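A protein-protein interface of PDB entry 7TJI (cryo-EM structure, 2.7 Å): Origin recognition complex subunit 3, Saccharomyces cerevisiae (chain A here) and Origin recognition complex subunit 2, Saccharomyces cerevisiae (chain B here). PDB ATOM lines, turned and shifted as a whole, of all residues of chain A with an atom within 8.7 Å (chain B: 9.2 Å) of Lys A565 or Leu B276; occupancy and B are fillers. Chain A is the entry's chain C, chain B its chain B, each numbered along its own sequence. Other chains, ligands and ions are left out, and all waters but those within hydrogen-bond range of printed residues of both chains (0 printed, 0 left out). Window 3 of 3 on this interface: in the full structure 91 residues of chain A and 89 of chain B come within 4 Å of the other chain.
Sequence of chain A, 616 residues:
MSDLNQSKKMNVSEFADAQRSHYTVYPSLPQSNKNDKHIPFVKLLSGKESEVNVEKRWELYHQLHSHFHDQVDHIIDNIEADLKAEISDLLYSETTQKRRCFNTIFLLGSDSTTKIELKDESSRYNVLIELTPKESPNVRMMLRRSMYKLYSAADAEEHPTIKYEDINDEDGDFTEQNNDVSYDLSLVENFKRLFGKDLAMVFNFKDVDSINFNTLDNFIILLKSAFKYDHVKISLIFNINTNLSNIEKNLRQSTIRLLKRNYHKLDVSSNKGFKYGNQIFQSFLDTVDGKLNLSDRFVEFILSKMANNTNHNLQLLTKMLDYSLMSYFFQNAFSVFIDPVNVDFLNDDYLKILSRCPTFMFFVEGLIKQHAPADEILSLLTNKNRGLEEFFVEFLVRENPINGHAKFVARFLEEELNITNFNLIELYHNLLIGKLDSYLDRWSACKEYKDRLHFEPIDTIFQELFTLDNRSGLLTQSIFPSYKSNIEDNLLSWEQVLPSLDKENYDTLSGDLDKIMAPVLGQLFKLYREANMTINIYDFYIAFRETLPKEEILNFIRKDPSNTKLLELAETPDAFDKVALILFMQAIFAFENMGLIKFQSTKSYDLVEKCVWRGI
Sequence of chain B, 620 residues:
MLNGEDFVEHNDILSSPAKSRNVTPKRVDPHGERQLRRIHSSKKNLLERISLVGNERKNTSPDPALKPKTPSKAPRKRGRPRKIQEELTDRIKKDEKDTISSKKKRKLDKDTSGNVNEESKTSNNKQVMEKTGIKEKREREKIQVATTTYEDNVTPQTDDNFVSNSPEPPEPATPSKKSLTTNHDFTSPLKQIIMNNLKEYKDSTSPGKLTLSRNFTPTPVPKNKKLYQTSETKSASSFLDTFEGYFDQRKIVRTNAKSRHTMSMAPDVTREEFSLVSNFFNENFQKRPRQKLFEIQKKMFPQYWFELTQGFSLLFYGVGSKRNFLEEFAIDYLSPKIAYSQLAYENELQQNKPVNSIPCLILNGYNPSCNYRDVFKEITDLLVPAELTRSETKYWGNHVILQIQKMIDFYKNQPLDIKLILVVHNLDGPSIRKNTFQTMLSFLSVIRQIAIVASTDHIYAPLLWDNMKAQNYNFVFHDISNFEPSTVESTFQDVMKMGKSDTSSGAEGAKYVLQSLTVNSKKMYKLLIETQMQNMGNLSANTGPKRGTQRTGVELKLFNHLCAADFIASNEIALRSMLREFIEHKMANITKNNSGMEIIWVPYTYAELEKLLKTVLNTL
The backbone carbonyl oxygen of Phe B280 sits at hydrogen-bond distance from the side-chain amide nitrogen of Asn B284.
ND2 of Asn B282 lies within hydrogen-bond range of O of Ser B278 (3.0 Å).
The side-chain hydroxyl of Ser B278 lies close to the backbone carbonyl oxygen of Phe B274 (3.2 Å).
The backbone carbonyl oxygen (O) of Leu A569 sits at hydrogen-bond distance from the side-chain hydroxyl (OG1) of Thr A572, at 3.2 Å.
The backbone NH of Thr B270 is in hydrogen-bond range of the side-chain carboxylate of Glu B273, 2.7 Å away.
Among the printed residues, merely in contact across the chains: Leu A569 with Glu B273 (3.4 Å), Ile A557 with Phe B280 (3.6 Å), Ile A582 with Phe B274 (3.6 Å), Leu A566 with Phe B280 (3.6 Å), Ile A582 with Ser B278 (3.7 Å), Leu A583 with Phe B281 (3.7 Å), Lys A565 with Leu B276 (3.7 Å), Leu A569 with Val B277 (3.7 Å), Ile A582 with Val B277 (3.7 Å), Leu A566 with Leu B276 (3.8 Å), Val A579 with Phe B281 (3.8 Å), Asn A563 with Leu B276 (3.9 Å) and Ile A557 with Phe B281 (3.9 Å).
No residue of chain B comes within 4 Å of Thr A564.
Of chain B, only Leu B276 (3.7 Å) comes within 4 Å of Lys A565.
Of chain B, only Leu B276 (3.8 Å) and Phe B280 (3.6 Å) come within 4 Å of Leu A566.
Printed residues of chain A within 4 Å of Glu B273: Leu A569 (3.4 Å).
Leu B276 touches three residues of chain A.
Of the printed residues of chain A, Ser B278 touches Ile A582 (3.7 Å).
Printed residues of chain A within 4 Å of Phe B280: Ile A557 and Leu A566.
Printed residues of chain B that touch a printed residue of chain A: Glu B273, Phe B274, Leu B276, Val B277, Ser B278, Phe B280 and Phe B281.
Hydrophobic or aromatic side chains of chain B that line the printed part of chain A: Phe B274, Leu B276, Val B277, Phe B280 and Phe B281.
Hydrophobic or aromatic side chains of chain A that line the printed part of chain B: Ile A557, Leu A566, Leu A569, Val A579, Ile A582 and Leu A583.
Along chain A the printed residues that touch a printed residue of chain B span positions 557 to 583.
Among the printed residues, no Asp or Glu carboxylate lies within 4 Å of a Lys or Arg side-chain nitrogen of the other chain.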
ATOM      1  N   ILE A 557     -11.030  18.647 -16.345  1.00  0.00           N
ATOM      2  CA  ILE A 557      -9.698  18.221 -16.768  1.00  0.00           C
ATOM      3  C   ILE A 557      -8.741  19.402 -16.942  1.00  0.00           C
ATOM      4  O   ILE A 557      -7.520  19.200 -16.969  1.00  0.00           O
ATOM      5  CB  ILE A 557      -9.795  17.356 -18.040  1.00  0.00           C
ATOM      6  CG1 ILE A 557      -8.714  16.276 -18.031  1.00  0.00           C
ATOM      7  CG2 ILE A 557      -9.688  18.187 -19.307  1.00  0.00           C
ATOM      8  CD1 ILE A 557      -9.050  15.067 -18.868  1.00  0.00           C
ATOM      9  N   ASP A 560      -6.818  21.272 -13.163  1.00  0.00           N
ATOM     10  CA  ASP A 560      -5.477  21.013 -12.660  1.00  0.00           C
ATOM     11  C   ASP A 560      -4.459  21.612 -13.621  1.00  0.00           C
ATOM     12  O   ASP A 560      -4.358  21.147 -14.766  1.00  0.00           O
ATOM     13  CB  ASP A 560      -5.239  19.513 -12.501  1.00  0.00           C
ATOM     14  CG  ASP A 560      -4.035  19.199 -11.631  1.00  0.00           C
ATOM     15  OD1 ASP A 560      -3.458  20.137 -11.040  1.00  0.00           O
ATOM     16  OD2 ASP A 560      -3.664  18.010 -11.539  1.00  0.00           O
ATOM     17  N   PRO A 561      -3.696  22.628 -13.219  1.00  0.00           N
ATOM     18  CA  PRO A 561      -2.700  23.226 -14.116  1.00  0.00           C
ATOM     19  C   PRO A 561      -1.312  22.606 -14.048  1.00  0.00           C
ATOM     20  O   PRO A 561      -0.419  23.065 -14.769  1.00  0.00           O
ATOM     21  CB  PRO A 561      -2.660  24.679 -13.625  1.00  0.00           C
ATOM     22  CG  PRO A 561      -2.899  24.561 -12.155  1.00  0.00           C
ATOM     23  CD  PRO A 561      -3.802  23.366 -11.946  1.00  0.00           C
ATOM     24  N   SER A 562      -1.104  21.588 -13.218  1.00  0.00           N
ATOM     25  CA  SER A 562       0.208  20.983 -13.040  1.00  0.00           C
ATOM     26  C   SER A 562       0.443  19.789 -13.957  1.00  0.00           C
ATOM     27  O   SER A 562       1.464  19.108 -13.814  1.00  0.00           O
ATOM     28  CB  SER A 562       0.398  20.559 -11.581  1.00  0.00           C
ATOM     29  OG  SER A 562       1.455  19.623 -11.457  1.00  0.00           O
ATOM     30  N   ASN A 563      -0.473  19.512 -14.883  1.00  0.00           N
ATOM     31  CA  ASN A 563      -0.347  18.390 -15.813  1.00  0.00           C
ATOM     32  C   ASN A 563      -0.255  18.948 -17.232  1.00  0.00           C
ATOM     33  O   ASN A 563      -1.276  19.282 -17.847  1.00  0.00           O
ATOM     34  CB  ASN A 563      -1.511  17.420 -15.654  1.00  0.00           C
ATOM     35  CG  ASN A 563      -1.109  15.986 -15.919  1.00  0.00           C
ATOM     36  OD1 ASN A 563      -0.371  15.702 -16.860  1.00  0.00           O
ATOM     37  ND2 ASN A 563      -1.570  15.078 -15.071  1.00  0.00           N
ATOM     38  N   THR A 564       0.977  19.032 -17.744  1.00  0.00           N
ATOM     39  CA  THR A 564       1.227  19.709 -19.015  1.00  0.00           C
ATOM     40  C   THR A 564       0.672  18.924 -20.200  1.00  0.00           C
ATOM     41  O   THR A 564       0.112  19.517 -21.128  1.00  0.00           O
ATOM     42  CB  THR A 564       2.726  19.965 -19.189  1.00  0.00           C
ATOM     43  OG1 THR A 564       3.027  20.155 -20.577  1.00  0.00           O
ATOM     44  CG2 THR A 564       3.551  18.807 -18.637  1.00  0.00           C
ATOM     45  N   LYS A 565       0.810  17.594 -20.187  1.00  0.00           N
ATOM     46  CA  LYS A 565       0.285  16.787 -21.286  1.00  0.00           C
ATOM     47  C   LYS A 565      -1.240  16.784 -21.293  1.00  0.00           C
ATOM     48  O   LYS A 565      -1.860  16.811 -22.364  1.00  0.00           O
ATOM     49  CB  LYS A 565       0.830  15.363 -21.199  1.00  0.00           C
ATOM     50  CG  LYS A 565       2.111  15.136 -21.991  1.00  0.00           C
ATOM     51  CD  LYS A 565       3.343  15.460 -21.165  1.00  0.00           C
ATOM     52  CE  LYS A 565       3.529  14.458 -20.038  1.00  0.00           C
ATOM     53  NZ  LYS A 565       4.784  14.705 -19.275  1.00  0.00           N
ATOM     54  N   LEU A 566      -1.856  16.786 -20.105  1.00  0.00           N
ATOM     55  CA  LEU A 566      -3.308  16.909 -20.006  1.00  0.00           C
ATOM     56  C   LEU A 566      -3.793  18.256 -20.523  1.00  0.00           C
ATOM     57  O   LEU A 566      -4.803  18.326 -21.235  1.00  0.00           O
ATOM     58  CB  LEU A 566      -3.758  16.720 -18.559  1.00  0.00           C
ATOM     59  CG  LEU A 566      -4.047  15.311 -18.055  1.00  0.00           C
ATOM     60  CD1 LEU A 566      -4.574  15.403 -16.647  1.00  0.00           C
ATOM     61  CD2 LEU A 566      -5.051  14.618 -18.954  1.00  0.00           C
ATOM     62  N   LEU A 567      -3.088  19.338 -20.173  1.00  0.00           N
ATOM     63  CA  LEU A 567      -3.475  20.658 -20.662  1.00  0.00           C
ATOM     64  C   LEU A 567      -3.231  20.802 -22.158  1.00  0.00           C
ATOM     65  O   LEU A 567      -3.936  21.566 -22.828  1.00  0.00           O
ATOM     66  CB  LEU A 567      -2.725  21.746 -19.891  1.00  0.00           C
ATOM     67  CG  LEU A 567      -3.183  22.034 -18.459  1.00  0.00           C
ATOM     68  CD1 LEU A 567      -2.627  23.368 -17.982  1.00  0.00           C
ATOM     69  CD2 LEU A 567      -4.700  22.012 -18.337  1.00  0.00           C
ATOM     70  N   GLU A 568      -2.236  20.091 -22.693  1.00  0.00           N
ATOM     71  CA  GLU A 568      -2.026  20.061 -24.137  1.00  0.00           C
ATOM     72  C   GLU A 568      -3.155  19.319 -24.843  1.00  0.00           C
ATOM     73  O   GLU A 568      -3.653  19.766 -25.882  1.00  0.00           O
ATOM     74  CB  GLU A 568      -0.676  19.416 -24.450  1.00  0.00           C
ATOM     75  CG  GLU A 568      -0.329  19.359 -25.927  1.00  0.00           C
ATOM     76  CD  GLU A 568       1.081  18.857 -26.172  1.00  0.00           C
ATOM     77  OE1 GLU A 568       1.710  18.360 -25.214  1.00  0.00           O
ATOM     78  OE2 GLU A 568       1.560  18.963 -27.320  1.00  0.00           O
ATOM     79  N   LEU A 569      -3.571  18.175 -24.290  1.00  0.00           N
ATOM     80  CA  LEU A 569      -4.638  17.384 -24.892  1.00  0.00           C
ATOM     81  C   LEU A 569      -6.000  18.065 -24.793  1.00  0.00           C
ATOM     82  O   LEU A 569      -6.804  17.948 -25.725  1.00  0.00           O
ATOM     83  CB  LEU A 569      -4.686  15.999 -24.237  1.00  0.00           C
ATOM     84  CG  LEU A 569      -5.892  15.085 -24.482  1.00  0.00           C
ATOM     85  CD1 LEU A 569      -5.716  14.267 -25.753  1.00  0.00           C
ATOM     86  CD2 LEU A 569      -6.130  14.185 -23.287  1.00  0.00           C
ATOM     87  N   ALA A 570      -6.261  18.800 -23.707  1.00  0.00           N
ATOM     88  CA  ALA A 570      -7.586  19.378 -23.498  1.00  0.00           C
ATOM     89  C   ALA A 570      -7.874  20.517 -24.470  1.00  0.00           C
ATOM     90  O   ALA A 570      -9.035  20.763 -24.816  1.00  0.00           O
ATOM     91  CB  ALA A 570      -7.721  19.858 -22.056  1.00  0.00           C
ATOM     92  N   GLU A 571      -6.838  21.223 -24.921  1.00  0.00           N
ATOM     93  CA  GLU A 571      -7.032  22.296 -25.888  1.00  0.00           C
ATOM     94  C   GLU A 571      -7.256  21.784 -27.306  1.00  0.00           C
ATOM     95  O   GLU A 571      -7.705  22.556 -28.160  1.00  0.00           O
ATOM     96  CB  GLU A 571      -5.837  23.252 -25.861  1.00  0.00           C
ATOM     97  CG  GLU A 571      -5.799  24.145 -24.631  1.00  0.00           C
ATOM     98  CD  GLU A 571      -4.600  25.072 -24.618  1.00  0.00           C
ATOM     99  OE1 GLU A 571      -3.725  24.928 -25.497  1.00  0.00           O
ATOM    100  OE2 GLU A 571      -4.533  25.946 -23.727  1.00  0.00           O
ATOM    101  N   THR A 572      -6.943  20.520 -27.574  1.00  0.00           N
ATOM    102  CA  THR A 572      -7.289  19.912 -28.851  1.00  0.00           C
ATOM    103  C   THR A 572      -8.808  19.735 -28.926  1.00  0.00           C
ATOM    104  O   THR A 572      -9.431  19.359 -27.929  1.00  0.00           O
ATOM    105  CB  THR A 572      -6.572  18.563 -28.987  1.00  0.00           C
ATOM    106  OG1 THR A 572      -5.269  18.666 -28.400  1.00  0.00           O
ATOM    107  CG2 THR A 572      -6.385  18.172 -30.443  1.00  0.00           C
ATOM    108  N   VAL A 579     -11.392  11.553 -24.344  1.00  0.00           N
ATOM    109  CA  VAL A 579     -11.613  11.257 -22.931  1.00  0.00           C
ATOM    110  C   VAL A 579     -12.758  10.265 -22.762  1.00  0.00           C
ATOM    111  O   VAL A 579     -12.653   9.302 -21.981  1.00  0.00           O
ATOM    112  CB  VAL A 579     -11.865  12.577 -22.172  1.00  0.00           C
ATOM    113  CG1 VAL A 579     -12.699  12.368 -20.908  1.00  0.00           C
ATOM    114  CG2 VAL A 579     -10.544  13.257 -21.839  1.00  0.00           C
ATOM    115  N   ILE A 582     -11.560   6.783 -23.786  1.00  0.00           N
ATOM    116  CA  ILE A 582     -10.662   6.153 -22.816  1.00  0.00           C
ATOM    117  C   ILE A 582     -11.450   5.607 -21.626  1.00  0.00           C
ATOM    118  O   ILE A 582     -11.266   4.448 -21.215  1.00  0.00           O
ATOM    119  CB  ILE A 582      -9.568   7.143 -22.374  1.00  0.00           C
ATOM    120  CG1 ILE A 582      -8.593   7.428 -23.522  1.00  0.00           C
ATOM    121  CG2 ILE A 582      -8.802   6.608 -21.180  1.00  0.00           C
ATOM    122  CD1 ILE A 582      -8.181   6.213 -24.328  1.00  0.00           C
ATOM    123  N   LEU A 583     -12.379   6.418 -21.096  1.00  0.00           N
ATOM    124  CA  LEU A 583     -13.234   5.965 -19.999  1.00  0.00           C
ATOM    125  C   LEU A 583     -14.125   4.803 -20.423  1.00  0.00           C
ATOM    126  O   LEU A 583     -14.277   3.819 -19.679  1.00  0.00           O
ATOM    127  CB  LEU A 583     -14.082   7.128 -19.486  1.00  0.00           C
ATOM    128  CG  LEU A 583     -13.312   8.322 -18.929  1.00  0.00           C
ATOM    129  CD1 LEU A 583     -14.261   9.445 -18.542  1.00  0.00           C
ATOM    130  CD2 LEU A 583     -12.458   7.900 -17.753  1.00  0.00           C
ATOM    131  N   THR B 270      -3.239   7.314 -28.886  1.00  0.00           N
ATOM    132  CA  THR B 270      -1.990   6.641 -28.575  1.00  0.00           C
ATOM    133  C   THR B 270      -2.132   5.888 -27.255  1.00  0.00           C
ATOM    134  O   THR B 270      -3.112   6.043 -26.523  1.00  0.00           O
ATOM    135  CB  THR B 270      -0.833   7.637 -28.514  1.00  0.00           C
ATOM    136  OG1 THR B 270      -1.106   8.635 -27.525  1.00  0.00           O
ATOM    137  CG2 THR B 270      -0.637   8.309 -29.865  1.00  0.00           C
ATOM    138  N   ARG B 271      -1.135   5.056 -26.953  1.00  0.00           N
ATOM    139  CA  ARG B 271      -1.242   4.172 -25.797  1.00  0.00           C
ATOM    140  C   ARG B 271      -1.052   4.922 -24.481  1.00  0.00           C
ATOM    141  O   ARG B 271      -1.736   4.625 -23.496  1.00  0.00           O
ATOM    142  CB  ARG B 271      -0.231   3.030 -25.918  1.00  0.00           C
ATOM    143  CG  ARG B 271      -0.396   1.927 -24.885  1.00  0.00           C
ATOM    144  CD  ARG B 271       0.707   1.951 -23.839  1.00  0.00           C
ATOM    145  NE  ARG B 271       0.948   0.628 -23.275  1.00  0.00           N
ATOM    146  CZ  ARG B 271       0.246   0.093 -22.286  1.00  0.00           C
ATOM    147  NH1 ARG B 271      -0.750   0.747 -21.711  1.00  0.00           N
ATOM    148  NH2 ARG B 271       0.553  -1.129 -21.859  1.00  0.00           N
ATOM    149  N   GLU B 272      -0.139   5.896 -24.443  1.00  0.00           N
ATOM    150  CA  GLU B 272       0.222   6.526 -23.174  1.00  0.00           C
ATOM    151  C   GLU B 272      -0.789   7.580 -22.724  1.00  0.00           C
ATOM    152  O   GLU B 272      -0.920   7.829 -21.518  1.00  0.00           O
ATOM    153  CB  GLU B 272       1.636   7.121 -23.262  1.00  0.00           C
ATOM    154  CG  GLU B 272       1.753   8.532 -23.837  1.00  0.00           C
ATOM    155  CD  GLU B 272       1.241   8.636 -25.263  1.00  0.00           C
ATOM    156  OE1 GLU B 272       1.650   7.810 -26.105  1.00  0.00           O
ATOM    157  OE2 GLU B 272       0.421   9.538 -25.536  1.00  0.00           O
ATOM    158  N   GLU B 273      -1.525   8.199 -23.654  1.00  0.00           N
ATOM    159  CA  GLU B 273      -2.538   9.159 -23.237  1.00  0.00           C
ATOM    160  C   GLU B 273      -3.755   8.474 -22.632  1.00  0.00           C
ATOM    161  O   GLU B 273      -4.459   9.098 -21.831  1.00  0.00           O
ATOM    162  CB  GLU B 273      -2.951  10.059 -24.405  1.00  0.00           C
ATOM    163  CG  GLU B 273      -3.638   9.362 -25.557  1.00  0.00           C
ATOM    164  CD  GLU B 273      -3.799  10.275 -26.754  1.00  0.00           C
ATOM    165  OE1 GLU B 273      -3.829  11.508 -26.560  1.00  0.00           O
ATOM    166  OE2 GLU B 273      -3.878   9.765 -27.890  1.00  0.00           O
ATOM    167  N   PHE B 274      -3.987   7.201 -22.980  1.00  0.00           N
ATOM    168  CA  PHE B 274      -4.943   6.373 -22.249  1.00  0.00           C
ATOM    169  C   PHE B 274      -4.559   6.274 -20.779  1.00  0.00           C
ATOM    170  O   PHE B 274      -5.401   6.463 -19.895  1.00  0.00           O
ATOM    171  CB  PHE B 274      -5.017   4.978 -22.886  1.00  0.00           C
ATOM    172  CG  PHE B 274      -5.358   3.875 -21.915  1.00  0.00           C
ATOM    173  CD1 PHE B 274      -6.648   3.734 -21.421  1.00  0.00           C
ATOM    174  CD2 PHE B 274      -4.386   2.972 -21.501  1.00  0.00           C
ATOM    175  CE1 PHE B 274      -6.958   2.732 -20.525  1.00  0.00           C
ATOM    176  CE2 PHE B 274      -4.692   1.965 -20.605  1.00  0.00           C
ATOM    177  CZ  PHE B 274      -5.980   1.847 -20.118  1.00  0.00           C
ATOM    178  N   SER B 275      -3.281   5.989 -20.505  1.00  0.00           N
ATOM    179  CA  SER B 275      -2.813   5.863 -19.127  1.00  0.00           C
ATOM    180  C   SER B 275      -2.868   7.198 -18.396  1.00  0.00           C
ATOM    181  O   SER B 275      -3.218   7.245 -17.213  1.00  0.00           O
ATOM    182  CB  SER B 275      -1.393   5.299 -19.106  1.00  0.00           C
ATOM    183  OG  SER B 275      -0.788   5.488 -17.840  1.00  0.00           O
ATOM    184  N   LEU B 276      -2.562   8.290 -19.101  1.00  0.00           N
ATOM    185  CA  LEU B 276      -2.615   9.621 -18.497  1.00  0.00           C
ATOM    186  C   LEU B 276      -4.044  10.019 -18.126  1.00  0.00           C
ATOM    187  O   LEU B 276      -4.306  10.467 -16.996  1.00  0.00           O
ATOM    188  CB  LEU B 276      -2.003  10.636 -19.463  1.00  0.00           C
ATOM    189  CG  LEU B 276      -1.724  12.052 -18.973  1.00  0.00           C
ATOM    190  CD1 LEU B 276      -0.342  12.133 -18.356  1.00  0.00           C
ATOM    191  CD2 LEU B 276      -1.857  13.018 -20.131  1.00  0.00           C
ATOM    192  N   VAL B 277      -4.986   9.845 -19.064  1.00  0.00           N
ATOM    193  CA  VAL B 277      -6.384  10.189 -18.822  1.00  0.00           C
ATOM    194  C   VAL B 277      -6.983   9.284 -17.748  1.00  0.00           C
ATOM    195  O   VAL B 277      -7.733   9.749 -16.877  1.00  0.00           O
ATOM    196  CB  VAL B 277      -7.171  10.125 -20.148  1.00  0.00           C
ATOM    197  CG1 VAL B 277      -8.684  10.118 -19.922  1.00  0.00           C
ATOM    198  CG2 VAL B 277      -6.794  11.294 -21.030  1.00  0.00           C
ATOM    199  N   SER B 278      -6.624   7.994 -17.762  1.00  0.00           N
ATOM    200  CA  SER B 278      -7.095   7.066 -16.740  1.00  0.00           C
ATOM    201  C   SER B 278      -6.551   7.422 -15.365  1.00  0.00           C
ATOM    202  O   SER B 278      -7.291   7.373 -14.380  1.00  0.00           O
ATOM    203  CB  SER B 278      -6.712   5.635 -17.111  1.00  0.00           C
ATOM    204  OG  SER B 278      -7.650   5.075 -18.009  1.00  0.00           O
ATOM    205  N   ASN B 279      -5.273   7.808 -15.279  1.00  0.00           N
ATOM    206  CA  ASN B 279      -4.692   8.181 -13.993  1.00  0.00           C
ATOM    207  C   ASN B 279      -5.363   9.423 -13.421  1.00  0.00           C
ATOM    208  O   ASN B 279      -5.696   9.455 -12.231  1.00  0.00           O
ATOM    209  CB  ASN B 279      -3.187   8.401 -14.137  1.00  0.00           C
ATOM    210  CG  ASN B 279      -2.393   7.125 -13.950  1.00  0.00           C
ATOM    211  OD1 ASN B 279      -1.573   6.762 -14.793  1.00  0.00           O
ATOM    212  ND2 ASN B 279      -2.634   6.435 -12.842  1.00  0.00           N
ATOM    213  N   PHE B 280      -5.636  10.421 -14.272  1.00  0.00           N
ATOM    214  CA  PHE B 280      -6.341  11.613 -13.799  1.00  0.00           C
ATOM    215  C   PHE B 280      -7.773  11.295 -13.372  1.00  0.00           C
ATOM    216  O   PHE B 280      -8.195  11.651 -12.261  1.00  0.00           O
ATOM    217  CB  PHE B 280      -6.353  12.690 -14.881  1.00  0.00           C
ATOM    218  CG  PHE B 280      -7.040  13.951 -14.456  1.00  0.00           C
ATOM    219  CD1 PHE B 280      -6.442  14.799 -13.540  1.00  0.00           C
ATOM    220  CD2 PHE B 280      -8.294  14.279 -14.949  1.00  0.00           C
ATOM    221  CE1 PHE B 280      -7.072  15.956 -13.129  1.00  0.00           C
ATOM    222  CE2 PHE B 280      -8.928  15.439 -14.542  1.00  0.00           C
ATOM    223  CZ  PHE B 280      -8.314  16.277 -13.632  1.00  0.00           C
ATOM    224  N   PHE B 281      -8.526  10.600 -14.230  1.00  0.00           N
ATOM    225  CA  PHE B 281      -9.947  10.384 -13.977  1.00  0.00           C
ATOM    226  C   PHE B 281     -10.189   9.327 -12.909  1.00  0.00           C
ATOM    227  O   PHE B 281     -11.314   9.191 -12.420  1.00  0.00           O
ATOM    228  CB  PHE B 281     -10.657   9.993 -15.271  1.00  0.00           C
ATOM    229  CG  PHE B 281     -11.564  11.057 -15.810  1.00  0.00           C
ATOM    230  CD1 PHE B 281     -12.874  11.155 -15.369  1.00  0.00           C
ATOM    231  CD2 PHE B 281     -11.109  11.959 -16.757  1.00  0.00           C
ATOM    232  CE1 PHE B 281     -13.717  12.135 -15.864  1.00  0.00           C
ATOM    233  CE2 PHE B 281     -11.946  12.940 -17.258  1.00  0.00           C
ATOM    234  CZ  PHE B 281     -13.252  13.027 -16.809  1.00  0.00           C
ATOM    235  N   ASN B 282      -9.169   8.559 -12.545  1.00  0.00           N
ATOM    236  CA  ASN B 282      -9.296   7.632 -11.438  1.00  0.00           C
ATOM    237  C   ASN B 282      -8.666   8.153 -10.157  1.00  0.00           C
ATOM    238  O   ASN B 282      -8.945   7.607  -9.085  1.00  0.00           O
ATOM    239  CB  ASN B 282      -8.688   6.283 -11.829  1.00  0.00           C
ATOM    240  CG  ASN B 282      -9.390   5.661 -13.026  1.00  0.00           C
ATOM    241  OD1 ASN B 282     -10.553   5.959 -13.301  1.00  0.00           O
ATOM    242  ND2 ASN B 282      -8.680   4.815 -13.757  1.00  0.00           N
ATOM    243  N   GLU B 283      -7.835   9.194 -10.232  1.00  0.00           N
ATOM    244  CA  GLU B 283      -7.345   9.849  -9.031  1.00  0.00           C
ATOM    245  C   GLU B 283      -8.178  11.053  -8.617  1.00  0.00           C
ATOM    246  O   GLU B 283      -7.942  11.597  -7.533  1.00  0.00           O
ATOM    247  CB  GLU B 283      -5.889  10.288  -9.225  1.00  0.00           C
ATOM    248  CG  GLU B 283      -4.876   9.177  -9.018  1.00  0.00           C
ATOM    249  CD  GLU B 283      -4.797   8.723  -7.574  1.00  0.00           C
ATOM    250  OE1 GLU B 283      -4.898   9.582  -6.673  1.00  0.00           O
ATOM    251  OE2 GLU B 283      -4.635   7.508  -7.340  1.00  0.00           O
ATOM    252  N   ASN B 284      -9.132  11.493  -9.439  1.00  0.00           N
ATOM    253  CA  ASN B 284      -9.881  12.689  -9.064  1.00  0.00           C
ATOM    254  C   ASN B 284     -11.397  12.522  -9.104  1.00  0.00           C
ATOM    255  O   ASN B 284     -12.099  13.066  -8.246  1.00  0.00           O
ATOM    256  CB  ASN B 284      -9.462  13.855  -9.959  1.00  0.00           C
ATOM    257  CG  ASN B 284      -8.030  14.283  -9.715  1.00  0.00           C
ATOM    258  OD1 ASN B 284      -7.748  15.050  -8.797  1.00  0.00           O
ATOM    259  ND2 ASN B 284      -7.115  13.770 -10.524  1.00  0.00           N
